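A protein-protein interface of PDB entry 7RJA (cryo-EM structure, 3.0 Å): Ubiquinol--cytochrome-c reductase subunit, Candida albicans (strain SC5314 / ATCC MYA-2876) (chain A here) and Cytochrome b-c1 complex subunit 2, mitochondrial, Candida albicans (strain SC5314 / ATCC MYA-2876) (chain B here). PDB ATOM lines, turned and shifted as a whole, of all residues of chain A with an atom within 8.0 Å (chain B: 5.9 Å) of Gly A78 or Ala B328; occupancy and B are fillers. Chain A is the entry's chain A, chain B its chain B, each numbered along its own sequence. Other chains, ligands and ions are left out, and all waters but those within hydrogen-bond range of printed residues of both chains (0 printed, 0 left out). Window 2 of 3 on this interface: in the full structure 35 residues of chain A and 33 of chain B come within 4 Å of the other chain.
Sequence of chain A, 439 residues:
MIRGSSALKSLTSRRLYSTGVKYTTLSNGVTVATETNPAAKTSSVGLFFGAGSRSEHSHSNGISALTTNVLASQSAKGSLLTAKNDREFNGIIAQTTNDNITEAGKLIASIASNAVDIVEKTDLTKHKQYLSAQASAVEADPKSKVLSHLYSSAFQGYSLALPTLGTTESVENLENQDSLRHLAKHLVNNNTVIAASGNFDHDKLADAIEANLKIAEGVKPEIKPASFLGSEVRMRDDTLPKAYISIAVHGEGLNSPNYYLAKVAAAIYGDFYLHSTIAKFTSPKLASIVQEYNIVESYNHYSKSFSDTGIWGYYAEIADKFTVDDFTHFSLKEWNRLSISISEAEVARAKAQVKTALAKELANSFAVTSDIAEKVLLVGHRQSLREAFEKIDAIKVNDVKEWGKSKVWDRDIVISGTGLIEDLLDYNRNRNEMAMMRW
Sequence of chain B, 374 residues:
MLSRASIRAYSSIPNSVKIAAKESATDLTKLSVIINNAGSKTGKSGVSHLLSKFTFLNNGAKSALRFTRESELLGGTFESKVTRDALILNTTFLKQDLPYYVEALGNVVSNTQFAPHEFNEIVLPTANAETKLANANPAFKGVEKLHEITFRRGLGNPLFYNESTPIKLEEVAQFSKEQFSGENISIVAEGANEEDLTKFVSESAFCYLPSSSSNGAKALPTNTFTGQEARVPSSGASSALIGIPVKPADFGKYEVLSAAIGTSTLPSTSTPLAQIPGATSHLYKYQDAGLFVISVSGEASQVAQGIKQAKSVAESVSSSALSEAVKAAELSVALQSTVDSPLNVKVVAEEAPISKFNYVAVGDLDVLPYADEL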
ATOM      1  N   SER A  75     -24.749  21.799 -29.626  1.00  0.00           N
ATOM      2  CA  SER A  75     -24.666  20.365 -29.392  1.00  0.00           C
ATOM      3  C   SER A  75     -23.453  19.790 -30.109  1.00  0.00           C
ATOM      4  O   SER A  75     -23.242  20.044 -31.297  1.00  0.00           O
ATOM      5  CB  SER A  75     -25.942  19.681 -29.876  1.00  0.00           C
ATOM      6  OG  SER A  75     -27.092  20.331 -29.363  1.00  0.00           O
ATOM      7  N   ALA A  76     -22.660  19.004 -29.384  1.00  0.00           N
ATOM      8  CA  ALA A  76     -21.393  18.510 -29.899  1.00  0.00           C
ATOM      9  C   ALA A  76     -21.498  17.154 -30.581  1.00  0.00           C
ATOM     10  O   ALA A  76     -20.543  16.744 -31.247  1.00  0.00           O
ATOM     11  CB  ALA A  76     -20.370  18.418 -28.764  1.00  0.00           C
ATOM     12  N   LYS A  77     -22.619  16.451 -30.438  1.00  0.00           N
ATOM     13  CA  LYS A  77     -22.790  15.134 -31.049  1.00  0.00           C
ATOM     14  C   LYS A  77     -21.612  14.219 -30.726  1.00  0.00           C
ATOM     15  O   LYS A  77     -21.133  13.463 -31.572  1.00  0.00           O
ATOM     16  CB  LYS A  77     -22.979  15.252 -32.561  1.00  0.00           C
ATOM     17  CG  LYS A  77     -24.274  15.921 -32.977  1.00  0.00           C
ATOM     18  CD  LYS A  77     -24.439  15.902 -34.487  1.00  0.00           C
ATOM     19  CE  LYS A  77     -25.690  16.643 -34.922  1.00  0.00           C
ATOM     20  NZ  LYS A  77     -25.864  16.619 -36.399  1.00  0.00           N
ATOM     21  N   GLY A  78     -21.136  14.293 -29.487  1.00  0.00           N
ATOM     22  CA  GLY A  78     -20.073  13.439 -29.014  1.00  0.00           C
ATOM     23  C   GLY A  78     -18.678  14.008 -29.160  1.00  0.00           C
ATOM     24  O   GLY A  78     -17.762  13.543 -28.474  1.00  0.00           O
ATOM     25  N   SER A  79     -18.487  15.001 -30.023  1.00  0.00           N
ATOM     26  CA  SER A  79     -17.184  15.623 -30.179  1.00  0.00           C
ATOM     27  C   SER A  79     -16.932  16.587 -29.024  1.00  0.00           C
ATOM     28  O   SER A  79     -17.698  16.656 -28.059  1.00  0.00           O
ATOM     29  CB  SER A  79     -17.101  16.341 -31.523  1.00  0.00           C
ATOM     30  OG  SER A  79     -17.301  15.437 -32.594  1.00  0.00           O
ATOM     31  N   LEU A  80     -15.842  17.342 -29.116  1.00  0.00           N
ATOM     32  CA  LEU A  80     -15.496  18.364 -28.131  1.00  0.00           C
ATOM     33  C   LEU A  80     -15.418  19.694 -28.865  1.00  0.00           C
ATOM     34  O   LEU A  80     -14.407  20.002 -29.496  1.00  0.00           O
ATOM     35  CB  LEU A  80     -14.191  18.051 -27.435  1.00  0.00           C
ATOM     36  CG  LEU A  80     -13.817  19.083 -26.372  1.00  0.00           C
ATOM     37  CD1 LEU A  80     -14.805  19.003 -25.237  1.00  0.00           C
ATOM     38  CD2 LEU A  80     -12.400  18.892 -25.871  1.00  0.00           C
ATOM     39  N   LEU A  81     -16.490  20.472 -28.785  1.00  0.00           N
ATOM     40  CA  LEU A  81     -16.557  21.745 -29.485  1.00  0.00           C
ATOM     41  C   LEU A  81     -16.076  22.852 -28.555  1.00  0.00           C
ATOM     42  O   LEU A  81     -16.610  23.018 -27.455  1.00  0.00           O
ATOM     43  CB  LEU A  81     -17.990  22.007 -29.939  1.00  0.00           C
ATOM     44  CG  LEU A  81     -18.255  23.264 -30.762  1.00  0.00           C
ATOM     45  CD1 LEU A  81     -17.501  23.194 -32.068  1.00  0.00           C
ATOM     46  CD2 LEU A  81     -19.736  23.442 -31.011  1.00  0.00           C
ATOM     47  N   GLN A  95     -12.580  18.945 -31.482  1.00  0.00           N
ATOM     48  CA  GLN A  95     -11.675  17.831 -31.244  1.00  0.00           C
ATOM     49  C   GLN A  95     -12.458  16.528 -31.215  1.00  0.00           C
ATOM     50  O   GLN A  95     -13.611  16.491 -30.778  1.00  0.00           O
ATOM     51  CB  GLN A  95     -10.937  18.009 -29.922  1.00  0.00           C
ATOM     52  CG  GLN A  95     -10.239  19.331 -29.763  1.00  0.00           C
ATOM     53  CD  GLN A  95      -9.202  19.289 -28.668  1.00  0.00           C
ATOM     54  OE1 GLN A  95      -8.348  18.406 -28.643  1.00  0.00           O
ATOM     55  NE2 GLN A  95      -9.278  20.237 -27.744  1.00  0.00           N
ATOM     56  N   THR A  96     -11.831  15.453 -31.677  1.00  0.00           N
ATOM     57  CA  THR A  96     -12.474  14.148 -31.666  1.00  0.00           C
ATOM     58  C   THR A  96     -11.444  13.108 -32.068  1.00  0.00           C
ATOM     59  O   THR A  96     -10.426  13.429 -32.684  1.00  0.00           O
ATOM     60  CB  THR A  96     -13.678  14.105 -32.606  1.00  0.00           C
ATOM     61  OG1 THR A  96     -14.482  12.958 -32.304  1.00  0.00           O
ATOM     62  CG2 THR A  96     -13.224  14.041 -34.051  1.00  0.00           C
ATOM     63  N   THR A  97     -11.720  11.859 -31.714  1.00  0.00           N
ATOM     64  CA  THR A  97     -10.820  10.783 -32.082  1.00  0.00           C
ATOM     65  C   THR A  97     -10.774  10.640 -33.601  1.00  0.00           C
ATOM     66  O   THR A  97     -11.632  11.145 -34.327  1.00  0.00           O
ATOM     67  CB  THR A  97     -11.248   9.473 -31.424  1.00  0.00           C
ATOM     68  OG1 THR A  97     -10.396   8.412 -31.868  1.00  0.00           O
ATOM     69  CG2 THR A  97     -12.688   9.143 -31.761  1.00  0.00           C
ATOM     70  N   ASN A 100     -13.710   9.424 -35.964  1.00  0.00           N
ATOM     71  CA  ASN A 100     -14.895  10.267 -35.930  1.00  0.00           C
ATOM     72  C   ASN A 100     -14.697  11.601 -36.633  1.00  0.00           C
ATOM     73  O   ASN A 100     -15.656  12.374 -36.740  1.00  0.00           O
ATOM     74  CB  ASN A 100     -15.308  10.518 -34.477  1.00  0.00           C
ATOM     75  CG  ASN A 100     -16.672  11.152 -34.363  1.00  0.00           C
ATOM     76  OD1 ASN A 100     -17.667  10.599 -34.827  1.00  0.00           O
ATOM     77  ND2 ASN A 100     -16.730  12.322 -33.741  1.00  0.00           N
ATOM     78  N   ALA A 104     -17.243  15.180 -37.021  1.00  0.00           N
ATOM     79  CA  ALA A 104     -16.940  16.494 -36.473  1.00  0.00           C
ATOM     80  C   ALA A 104     -16.896  17.535 -37.578  1.00  0.00           C
ATOM     81  O   ALA A 104     -17.460  18.626 -37.436  1.00  0.00           O
ATOM     82  CB  ALA A 104     -15.614  16.459 -35.715  1.00  0.00           C
ATOM     83  N   LEU A 107     -20.262  18.531 -38.339  1.00  0.00           N
ATOM     84  CA  LEU A 107     -20.756  19.302 -37.208  1.00  0.00           C
ATOM     85  C   LEU A 107     -20.388  20.768 -37.366  1.00  0.00           C
ATOM     86  O   LEU A 107     -21.263  21.631 -37.498  1.00  0.00           O
ATOM     87  CB  LEU A 107     -20.201  18.738 -35.900  1.00  0.00           C
ATOM     88  CG  LEU A 107     -20.491  19.560 -34.645  1.00  0.00           C
ATOM     89  CD1 LEU A 107     -21.963  19.910 -34.560  1.00  0.00           C
ATOM     90  CD2 LEU A 107     -20.054  18.808 -33.407  1.00  0.00           C
ATOM     91  N   ALA B 259     -16.915  12.053 -18.821  1.00  0.00           N
ATOM     92  CA  ALA B 259     -17.116  12.775 -20.069  1.00  0.00           C
ATOM     93  C   ALA B 259     -18.585  13.104 -20.284  1.00  0.00           C
ATOM     94  O   ALA B 259     -18.907  14.108 -20.927  1.00  0.00           O
ATOM     95  CB  ALA B 259     -16.577  11.958 -21.239  1.00  0.00           C
ATOM     96  N   LEU B 266     -11.405  17.513 -21.000  1.00  0.00           N
ATOM     97  CA  LEU B 266     -12.215  18.098 -22.063  1.00  0.00           C
ATOM     98  C   LEU B 266     -12.832  19.394 -21.558  1.00  0.00           C
ATOM     99  O   LEU B 266     -13.990  19.405 -21.115  1.00  0.00           O
ATOM    100  CB  LEU B 266     -13.304  17.125 -22.517  1.00  0.00           C
ATOM    101  CG  LEU B 266     -12.866  15.704 -22.863  1.00  0.00           C
ATOM    102  CD1 LEU B 266     -14.070  14.893 -23.293  1.00  0.00           C
ATOM    103  CD2 LEU B 266     -11.809  15.702 -23.952  1.00  0.00           C
ATOM    104  N   GLU B 324     -24.208   8.384 -25.539  1.00  0.00           N
ATOM    105  CA  GLU B 324     -23.741   9.453 -26.414  1.00  0.00           C
ATOM    106  C   GLU B 324     -22.362   9.945 -26.004  1.00  0.00           C
ATOM    107  O   GLU B 324     -21.567  10.351 -26.859  1.00  0.00           O
ATOM    108  CB  GLU B 324     -24.731  10.616 -26.398  1.00  0.00           C
ATOM    109  CG  GLU B 324     -24.363  11.748 -27.341  1.00  0.00           C
ATOM    110  CD  GLU B 324     -25.388  12.862 -27.338  1.00  0.00           C
ATOM    111  OE1 GLU B 324     -26.377  12.759 -26.583  1.00  0.00           O
ATOM    112  OE2 GLU B 324     -25.204  13.843 -28.087  1.00  0.00           O
ATOM    113  N   ALA B 325     -22.066   9.928 -24.709  1.00  0.00           N
ATOM    114  CA  ALA B 325     -20.782  10.393 -24.203  1.00  0.00           C
ATOM    115  C   ALA B 325     -19.656   9.388 -24.404  1.00  0.00           C
ATOM    116  O   ALA B 325     -18.525   9.671 -24.001  1.00  0.00           O
ATOM    117  CB  ALA B 325     -20.894  10.727 -22.716  1.00  0.00           C
ATOM    118  N   VAL B 326     -19.931   8.226 -24.999  1.00  0.00           N
ATOM    119  CA  VAL B 326     -18.885   7.223 -25.173  1.00  0.00           C
ATOM    120  C   VAL B 326     -17.771   7.761 -26.055  1.00  0.00           C
ATOM    121  O   VAL B 326     -16.583   7.571 -25.770  1.00  0.00           O
ATOM    122  CB  VAL B 326     -19.481   5.928 -25.753  1.00  0.00           C
ATOM    123  CG1 VAL B 326     -18.378   5.023 -26.271  1.00  0.00           C
ATOM    124  CG2 VAL B 326     -20.319   5.218 -24.708  1.00  0.00           C
ATOM    125  N   LYS B 327     -18.131   8.429 -27.150  1.00  0.00           N
ATOM    126  CA  LYS B 327     -17.115   8.932 -28.066  1.00  0.00           C
ATOM    127  C   LYS B 327     -16.295  10.040 -27.418  1.00  0.00           C
ATOM    128  O   LYS B 327     -15.076  10.114 -27.606  1.00  0.00           O
ATOM    129  CB  LYS B 327     -17.778   9.422 -29.351  1.00  0.00           C
ATOM    130  CG  LYS B 327     -16.813   9.781 -30.467  1.00  0.00           C
ATOM    131  CD  LYS B 327     -15.936   8.604 -30.891  1.00  0.00           C
ATOM    132  CE  LYS B 327     -16.739   7.447 -31.473  1.00  0.00           C
ATOM    133  NZ  LYS B 327     -17.342   7.786 -32.790  1.00  0.00           N
ATOM    134  N   ALA B 328     -16.947  10.909 -26.643  1.00  0.00           N
ATOM    135  CA  ALA B 328     -16.213  11.938 -25.917  1.00  0.00           C
ATOM    136  C   ALA B 328     -15.264  11.316 -24.904  1.00  0.00           C
ATOM    137  O   ALA B 328     -14.144  11.801 -24.711  1.00  0.00           O
ATOM    138  CB  ALA B 328     -17.188  12.887 -25.224  1.00  0.00           C
ATOM    139  N   ALA B 329     -15.696  10.245 -24.237  1.00  0.00           N
ATOM    140  CA  ALA B 329     -14.820   9.569 -23.288  1.00  0.00           C
ATOM    141  C   ALA B 329     -13.626   8.942 -23.990  1.00  0.00           C
ATOM    142  O   ALA B 329     -12.509   8.961 -23.464  1.00  0.00           O
ATOM    143  CB  ALA B 329     -15.603   8.512 -22.521  1.00  0.00           C
ATOM    144  N   GLU B 330     -13.845   8.362 -25.170  1.00  0.00           N
ATOM    145  CA  GLU B 330     -12.728   7.823 -25.938  1.00  0.00           C
ATOM    146  C   GLU B 330     -11.757   8.929 -26.325  1.00  0.00           C
ATOM    147  O   GLU B 330     -10.534   8.748 -26.266  1.00  0.00           O
ATOM    148  CB  GLU B 330     -13.245   7.097 -27.178  1.00  0.00           C
ATOM    149  CG  GLU B 330     -12.156   6.462 -28.022  1.00  0.00           C
ATOM    150  CD  GLU B 330     -11.433   5.345 -27.297  1.00  0.00           C
ATOM    151  OE1 GLU B 330     -12.036   4.735 -26.390  1.00  0.00           O
ATOM    152  OE2 GLU B 330     -10.260   5.078 -27.634  1.00  0.00           O
ATOM    153  N   LEU B 331     -12.284  10.089 -26.716  1.00  0.00           N
ATOM    154  CA  LEU B 331     -11.424  11.233 -26.995  1.00  0.00           C
ATOM    155  C   LEU B 331     -10.610  11.611 -25.766  1.00  0.00           C
ATOM    156  O   LEU B 331      -9.409  11.880 -25.860  1.00  0.00           O
ATOM    157  CB  LEU B 331     -12.266  12.420 -27.460  1.00  0.00           C
ATOM    158  CG  LEU B 331     -11.562  13.778 -27.466  1.00  0.00           C
ATOM    159  CD1 LEU B 331     -10.428  13.776 -28.463  1.00  0.00           C
ATOM    160  CD2 LEU B 331     -12.544  14.882 -27.782  1.00  0.00           C
ATOM    161  N   SER B 332     -11.257  11.658 -24.602  1.00  0.00           N
ATOM    162  CA  SER B 332     -10.557  12.043 -23.382  1.00  0.00           C
ATOM    163  C   SER B 332      -9.456  11.049 -23.046  1.00  0.00           C
ATOM    164  O   SER B 332      -8.350  11.440 -22.654  1.00  0.00           O
ATOM    165  CB  SER B 332     -11.547  12.155 -22.227  1.00  0.00           C
ATOM    166  OG  SER B 332     -10.878  12.136 -20.983  1.00  0.00           O
ATOM    167  N   VAL B 333      -9.740   9.756 -23.193  1.00  0.00           N
ATOM    168  CA  VAL B 333      -8.720   8.745 -22.947  1.00  0.00           C
ATOM    169  C   VAL B 333      -7.557   8.917 -23.908  1.00  0.00           C
ATOM    170  O   VAL B 333      -6.394   8.817 -23.506  1.00  0.00           O
ATOM    171  CB  VAL B 333      -9.330   7.337 -23.050  1.00  0.00           C
ATOM    172  CG1 VAL B 333      -8.238   6.289 -23.090  1.00  0.00           C
ATOM    173  CG2 VAL B 333     -10.261   7.087 -21.884  1.00  0.00           C
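N of Ala B328 sits at hydrogen-bond distance from O of Gly A78, at 3.3 Å.
OD1 of Asn A100 sits at hydrogen-bond distance from NZ of Lys B327 (3.5 Å).
Lys B327 touches Gly A78 (C to O, 3.9 Å).
Leu A80 touches Leu B266 (CD1 to CB, 3.6 Å).
CD2 of Leu B331 touches CB of Leu A80, 3.6 Å away.
Leu B331 touches Gln A95 (CD2 to O, 3.6 Å).
Thr A96 touches Leu B331.
Thr A97 touches Lys B327.
N of Thr A97 touches CD1 of Leu B331, 3.99 Å away.
Gly A78 touches just these residues of chain B: Lys B327 and Ala B328.
Of chain A, only Gly A78 comes within 4 Å of Ala B328.
Of the printed residues of chain B, Thr A96 touches Leu B331.
Printed residues of chain A within 4 Å of Leu B266: Leu A80 (3.6 Å).
Printed residues of chain A within 4 Å of Leu B331: Leu A80, Gln A95, Thr A96 and Thr A97.
The nearest residue of chain A that does not touch Ala B328 is Ser A79 (4.7 Å).
The nearest printed residue of chain B that does not touch Gln A95 is Leu B266 (6.4 Å).
The side-chain hydroxyl (OG1) of Thr A96 lies within hydrogen-bond range of the side-chain amide nitrogen (ND2) of Asn A100.
OG of Ser A79 sits at hydrogen-bond distance from ND2 of Asn A100, at 3.4 Å.
The backbone carbonyl oxygen of Leu A80 lies within hydrogen-bond range of the backbone NH of Gln A95.
Of the 12 printed residues of chain B, 4 touch a printed residue of chain A.
Printed residues of chain B that touch a printed residue of chain A: Leu B266, Lys B327, Ala B328 and Leu B331.
Hydrophobic or aromatic side chains of chain B that line the printed part of chain A: Leu B266, Ala B328 and Leu B331.
Among the printed residues, no Asp or Glu carboxylate lies within 4 Å of a Lys or Arg side-chain nitrogen of the other chain.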
